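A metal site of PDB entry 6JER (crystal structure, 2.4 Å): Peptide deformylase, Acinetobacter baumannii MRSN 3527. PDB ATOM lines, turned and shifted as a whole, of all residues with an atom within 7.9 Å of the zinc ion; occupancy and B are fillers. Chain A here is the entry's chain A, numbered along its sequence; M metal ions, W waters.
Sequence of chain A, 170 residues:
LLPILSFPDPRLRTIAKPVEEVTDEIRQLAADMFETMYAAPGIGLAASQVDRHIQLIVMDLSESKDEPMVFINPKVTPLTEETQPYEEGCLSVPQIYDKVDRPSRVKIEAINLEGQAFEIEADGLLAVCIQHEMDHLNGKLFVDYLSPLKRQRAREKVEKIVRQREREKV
A ring nitrogen (ND1) of His 132 lies within hydrogen-bond range of the side-chain carboxylate (OE1) of Glu 88 (2.7 Å). The side-chain sulfur (SG) of Cys 90 lies close to the side-chain amide nitrogen (NE2) of Gln 49 (3.6 Å). N of Ser 92 sits close to SG of Cys 90, at 3.3 Å. The side-chain carboxylate (OE1) of Glu 133 lies close to the side-chain amide oxygen (OE1) of Gln 49 (3.2 Å). NE2 of Gln 49 sits at hydrogen-bond distance from OG of Ser 92 (3.3 Å). N of Ala 46 sits at hydrogen-bond distance from OE1 of Gln 49 (2.9 Å).
NE2 of Gln 49 touches the zinc ion, 3.5 Å away. Four residues have an atom within 4 Å of the zinc ion: Gln 49, Cys 90, His 132 and His 136. The nearest printed residue that does not touch the zinc ion is Glu 133 (4.3 Å).
The zinc ion is bound by a ring nitrogen (NE2) of His 136 (2.0 Å), a ring nitrogen (NE2) of His 132 (2.1 Å) and the side-chain sulfur (SG) of Cys 90 (2.3 Å).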
ATOM      1  N   LEU A  12     -25.941  12.525  -7.484  1.00  0.00           N
ATOM      2  CA  LEU A  12     -26.529  13.363  -8.568  1.00  0.00           C
ATOM      3  C   LEU A  12     -28.046  13.440  -8.403  1.00  0.00           C
ATOM      4  O   LEU A  12     -28.670  14.289  -9.038  1.00  0.00           O
ATOM      5  CB  LEU A  12     -26.175  12.799  -9.941  1.00  0.00           C
ATOM      6  CG  LEU A  12     -24.720  12.995 -10.382  1.00  0.00           C
ATOM      7  CD1 LEU A  12     -24.398  12.166 -11.614  1.00  0.00           C
ATOM      8  CD2 LEU A  12     -24.403  14.471 -10.636  1.00  0.00           C
ATOM      9  N   GLY A  44     -22.076  24.569 -19.326  1.00  0.00           N
ATOM     10  CA  GLY A  44     -23.006  24.611 -18.173  1.00  0.00           C
ATOM     11  C   GLY A  44     -22.593  23.643 -17.066  1.00  0.00           C
ATOM     12  O   GLY A  44     -21.993  22.625 -17.372  1.00  0.00           O
ATOM     13  N   LEU A  45     -22.813  24.012 -15.816  1.00  0.00           N
ATOM     14  CA  LEU A  45     -22.503  23.161 -14.645  1.00  0.00           C
ATOM     15  C   LEU A  45     -23.276  23.683 -13.424  1.00  0.00           C
ATOM     16  O   LEU A  45     -23.260  24.920 -13.206  1.00  0.00           O
ATOM     17  CB  LEU A  45     -21.000  23.167 -14.374  1.00  0.00           C
ATOM     18  CG  LEU A  45     -20.523  22.112 -13.369  1.00  0.00           C
ATOM     19  CD1 LEU A  45     -20.482  20.726 -14.005  1.00  0.00           C
ATOM     20  CD2 LEU A  45     -19.146  22.484 -12.843  1.00  0.00           C
ATOM     21  N   ALA A  46     -23.946  22.733 -12.738  1.00  0.00           N
ATOM     22  CA  ALA A  46     -24.691  22.870 -11.474  1.00  0.00           C
ATOM     23  C   ALA A  46     -23.791  22.398 -10.335  1.00  0.00           C
ATOM     24  O   ALA A  46     -22.941  21.522 -10.592  1.00  0.00           O
ATOM     25  CB  ALA A  46     -25.951  22.026 -11.576  1.00  0.00           C
ATOM     26  N   GLN A  49     -23.310  18.858  -9.428  1.00  0.00           N
ATOM     27  CA  GLN A  49     -22.420  18.011 -10.237  1.00  0.00           C
ATOM     28  C   GLN A  49     -21.036  17.965  -9.613  1.00  0.00           C
ATOM     29  O   GLN A  49     -20.322  17.009  -9.930  1.00  0.00           O
ATOM     30  CB  GLN A  49     -22.328  18.471 -11.682  1.00  0.00           C
ATOM     31  CG  GLN A  49     -23.658  18.307 -12.394  1.00  0.00           C
ATOM     32  CD  GLN A  49     -23.636  18.954 -13.753  1.00  0.00           C
ATOM     33  OE1 GLN A  49     -24.118  20.077 -13.921  1.00  0.00           O
ATOM     34  NE2 GLN A  49     -23.040  18.264 -14.715  1.00  0.00           N
ATOM     35  N   GLU A  88     -28.331  17.280 -26.569  1.00  0.00           N
ATOM     36  CA  GLU A  88     -27.773  17.711 -25.263  1.00  0.00           C
ATOM     37  C   GLU A  88     -26.581  16.838 -24.895  1.00  0.00           C
ATOM     38  O   GLU A  88     -26.566  15.670 -25.259  1.00  0.00           O
ATOM     39  CB  GLU A  88     -28.826  17.679 -24.158  1.00  0.00           C
ATOM     40  CG  GLU A  88     -29.911  18.722 -24.356  1.00  0.00           C
ATOM     41  CD  GLU A  88     -30.782  18.932 -23.136  1.00  0.00           C
ATOM     42  OE1 GLU A  88     -30.295  18.672 -22.037  1.00  0.00           O
ATOM     43  OE2 GLU A  88     -31.946  19.329 -23.291  1.00  0.00           O
ATOM     44  N   GLY A  89     -25.634  17.431 -24.195  1.00  0.00           N
ATOM     45  CA  GLY A  89     -24.546  16.715 -23.517  1.00  0.00           C
ATOM     46  C   GLY A  89     -24.573  17.052 -22.037  1.00  0.00           C
ATOM     47  O   GLY A  89     -25.491  17.796 -21.610  1.00  0.00           O
ATOM     48  N   CYS A  90     -23.612  16.511 -21.283  1.00  0.00           N
ATOM     49  CA  CYS A  90     -23.502  16.686 -19.820  1.00  0.00           C
ATOM     50  C   CYS A  90     -22.163  16.109 -19.372  1.00  0.00           C
ATOM     51  O   CYS A  90     -21.860  14.944 -19.672  1.00  0.00           O
ATOM     52  CB  CYS A  90     -24.664  16.044 -19.061  1.00  0.00           C
ATOM     53  SG  CYS A  90     -24.598  16.342 -17.273  1.00  0.00           S
ATOM     54  N   LEU A  91     -21.397  16.961 -18.703  1.00  0.00           N
ATOM     55  CA  LEU A  91     -20.134  16.655 -18.004  1.00  0.00           C
ATOM     56  C   LEU A  91     -20.321  15.514 -16.976  1.00  0.00           C
ATOM     57  O   LEU A  91     -19.319  14.832 -16.704  1.00  0.00           O
ATOM     58  CB  LEU A  91     -19.711  17.970 -17.361  1.00  0.00           C
ATOM     59  CG  LEU A  91     -19.285  19.022 -18.367  1.00  0.00           C
ATOM     60  CD1 LEU A  91     -18.726  20.245 -17.652  1.00  0.00           C
ATOM     61  CD2 LEU A  91     -18.257  18.449 -19.353  1.00  0.00           C
ATOM     62  N   SER A  92     -21.548  15.284 -16.482  1.00  0.00           N
ATOM     63  CA  SER A  92     -21.895  14.192 -15.541  1.00  0.00           C
ATOM     64  C   SER A  92     -22.380  12.956 -16.297  1.00  0.00           C
ATOM     65  O   SER A  92     -22.501  11.904 -15.631  1.00  0.00           O
ATOM     66  CB  SER A  92     -22.905  14.601 -14.506  1.00  0.00           C
ATOM     67  OG  SER A  92     -22.286  15.340 -13.453  1.00  0.00           O
ATOM     68  N   VAL A  93     -22.657  13.071 -17.592  1.00  0.00           N
ATOM     69  CA  VAL A  93     -22.759  11.897 -18.522  1.00  0.00           C
ATOM     70  C   VAL A  93     -21.755  12.086 -19.656  1.00  0.00           C
ATOM     71  O   VAL A  93     -22.107  12.292 -20.809  1.00  0.00           O
ATOM     72  CB  VAL A  93     -24.183  11.706 -19.076  1.00  0.00           C
ATOM     73  CG1 VAL A  93     -24.355  10.306 -19.648  1.00  0.00           C
ATOM     74  CG2 VAL A  93     -25.243  11.974 -18.008  1.00  0.00           C
ATOM     75  N   ARG A 102     -37.581  20.130 -24.959  1.00  0.00           N
ATOM     76  CA  ARG A 102     -37.866  21.046 -23.825  1.00  0.00           C
ATOM     77  C   ARG A 102     -38.603  22.281 -24.337  1.00  0.00           C
ATOM     78  O   ARG A 102     -38.376  22.705 -25.458  1.00  0.00           O
ATOM     79  CB  ARG A 102     -36.573  21.489 -23.154  1.00  0.00           C
ATOM     80  CG  ARG A 102     -35.764  20.359 -22.540  1.00  0.00           C
ATOM     81  CD  ARG A 102     -34.551  20.952 -21.859  1.00  0.00           C
ATOM     82  NE  ARG A 102     -33.539  19.963 -21.503  1.00  0.00           N
ATOM     83  CZ  ARG A 102     -33.548  19.242 -20.384  1.00  0.00           C
ATOM     84  NH1 ARG A 102     -34.519  19.395 -19.492  1.00  0.00           N
ATOM     85  NH2 ARG A 102     -32.579  18.379 -20.155  1.00  0.00           N
ATOM     86  N   CYS A 129     -30.185  25.220 -21.906  1.00  0.00           N
ATOM     87  CA  CYS A 129     -29.141  25.073 -20.885  1.00  0.00           C
ATOM     88  C   CYS A 129     -29.705  25.367 -19.491  1.00  0.00           C
ATOM     89  O   CYS A 129     -29.330  24.574 -18.620  1.00  0.00           O
ATOM     90  CB  CYS A 129     -27.905  25.910 -21.203  1.00  0.00           C
ATOM     91  SG  CYS A 129     -26.394  25.078 -20.685  1.00  0.00           S
ATOM     92  N   HIS A 132     -31.854  22.309 -18.400  1.00  0.00           N
ATOM     93  CA  HIS A 132     -30.925  21.170 -18.142  1.00  0.00           C
ATOM     94  C   HIS A 132     -30.287  21.359 -16.768  1.00  0.00           C
ATOM     95  O   HIS A 132     -30.285  20.429 -16.001  1.00  0.00           O
ATOM     96  CB  HIS A 132     -29.867  21.072 -19.263  1.00  0.00           C
ATOM     97  CG  HIS A 132     -28.843  19.993 -19.059  1.00  0.00           C
ATOM     98  ND1 HIS A 132     -28.876  18.775 -19.748  1.00  0.00           N
ATOM     99  CD2 HIS A 132     -27.759  19.940 -18.252  1.00  0.00           C
ATOM    100  CE1 HIS A 132     -27.876  18.022 -19.345  1.00  0.00           C
ATOM    101  NE2 HIS A 132     -27.164  18.726 -18.435  1.00  0.00           N
ATOM    102  N   GLU A 133     -29.778  22.547 -16.446  1.00  0.00           N
ATOM    103  CA  GLU A 133     -29.072  22.782 -15.152  1.00  0.00           C
ATOM    104  C   GLU A 133     -30.061  22.796 -13.999  1.00  0.00           C
ATOM    105  O   GLU A 133     -29.692  22.323 -12.899  1.00  0.00           O
ATOM    106  CB  GLU A 133     -28.234  24.059 -15.194  1.00  0.00           C
ATOM    107  CG  GLU A 133     -27.213  24.053 -16.292  1.00  0.00           C
ATOM    108  CD  GLU A 133     -26.320  22.840 -16.375  1.00  0.00           C
ATOM    109  OE1 GLU A 133     -26.051  22.234 -15.316  1.00  0.00           O
ATOM    110  OE2 GLU A 133     -25.878  22.513 -17.513  1.00  0.00           O
ATOM    111  N   ASP A 135     -32.752  20.983 -13.785  1.00  0.00           N
ATOM    112  CA  ASP A 135     -33.009  19.552 -13.525  1.00  0.00           C
ATOM    113  C   ASP A 135     -31.955  19.065 -12.542  1.00  0.00           C
ATOM    114  O   ASP A 135     -32.325  18.383 -11.584  1.00  0.00           O
ATOM    115  CB  ASP A 135     -33.078  18.757 -14.824  1.00  0.00           C
ATOM    116  CG  ASP A 135     -34.424  18.851 -15.513  1.00  0.00           C
ATOM    117  OD1 ASP A 135     -35.333  19.507 -14.943  1.00  0.00           O
ATOM    118  OD2 ASP A 135     -34.566  18.251 -16.586  1.00  0.00           O
ATOM    119  N   HIS A 136     -30.670  19.394 -12.761  1.00  0.00           N
ATOM    120  CA  HIS A 136     -29.580  18.915 -11.867  1.00  0.00           C
ATOM    121  C   HIS A 136     -29.944  19.273 -10.426  1.00  0.00           C
ATOM    122  O   HIS A 136     -29.882  18.396  -9.549  1.00  0.00           O
ATOM    123  CB  HIS A 136     -28.214  19.461 -12.253  1.00  0.00           C
ATOM    124  CG  HIS A 136     -27.595  18.773 -13.410  1.00  0.00           C
ATOM    125  ND1 HIS A 136     -27.120  17.497 -13.310  1.00  0.00           N
ATOM    126  CD2 HIS A 136     -27.287  19.203 -14.652  1.00  0.00           C
ATOM    127  CE1 HIS A 136     -26.631  17.122 -14.474  1.00  0.00           C
ATOM    128  NE2 HIS A 136     -26.697  18.146 -15.313  1.00  0.00           N
ATOM    129  N   LYS A 140     -32.357  15.485 -11.402  1.00  0.00           N
ATOM    130  CA  LYS A 140     -32.763  14.915 -12.705  1.00  0.00           C
ATOM    131  C   LYS A 140     -31.610  15.050 -13.706  1.00  0.00           C
ATOM    132  O   LYS A 140     -30.919  16.095 -13.675  1.00  0.00           O
ATOM    133  CB  LYS A 140     -33.996  15.658 -13.226  1.00  0.00           C
ATOM    134  CG  LYS A 140     -35.334  15.087 -12.780  1.00  0.00           C
ATOM    135  CD  LYS A 140     -36.429  15.289 -13.822  1.00  0.00           C
ATOM    136  CE  LYS A 140     -36.431  14.230 -14.903  1.00  0.00           C
ATOM    137  NZ  LYS A 140     -37.393  14.525 -15.994  1.00  0.00           N
ATOM    138  N   LEU A 141     -31.421  14.029 -14.561  1.00  0.00           N
ATOM    139  CA  LEU A 141     -30.357  13.989 -15.609  1.00  0.00           C
ATOM    140  C   LEU A 141     -31.006  13.842 -16.978  1.00  0.00           C
ATOM    141  O   LEU A 141     -32.021  13.129 -17.066  1.00  0.00           O
ATOM    142  CB  LEU A 141     -29.436  12.792 -15.314  1.00  0.00           C
ATOM    143  CG  LEU A 141     -28.891  12.757 -13.896  1.00  0.00           C
ATOM    144  CD1 LEU A 141     -28.079  11.508 -13.628  1.00  0.00           C
ATOM    145  CD2 LEU A 141     -28.065  14.008 -13.650  1.00  0.00           C
ATOM    146  N   PHE A 142     -30.430  14.440 -18.019  1.00  0.00           N
ATOM    147  CA  PHE A 142     -31.060  14.459 -19.369  1.00  0.00           C
ATOM    148  C   PHE A 142     -31.272  13.027 -19.836  1.00  0.00           C
ATOM    149  O   PHE A 142     -32.117  12.824 -20.689  1.00  0.00           O
ATOM    150  CB  PHE A 142     -30.234  15.253 -20.389  1.00  0.00           C
ATOM    151  CG  PHE A 142     -29.109  14.518 -21.071  1.00  0.00           C
ATOM    152  CD1 PHE A 142     -27.825  14.542 -20.546  1.00  0.00           C
ATOM    153  CD2 PHE A 142     -29.331  13.801 -22.247  1.00  0.00           C
ATOM    154  CE1 PHE A 142     -26.791  13.874 -21.181  1.00  0.00           C
ATOM    155  CE2 PHE A 142     -28.289  13.145 -22.881  1.00  0.00           C
ATOM    156  CZ  PHE A 142     -27.012  13.172 -22.351  1.00  0.00           C
HETATM  157 ZN    ZN M   1     -25.723  18.277 -17.001  1.00  0.00          ZN
HETATM  158  O   HOH W   1     -27.909  15.602 -17.426  1.00  0.00           O
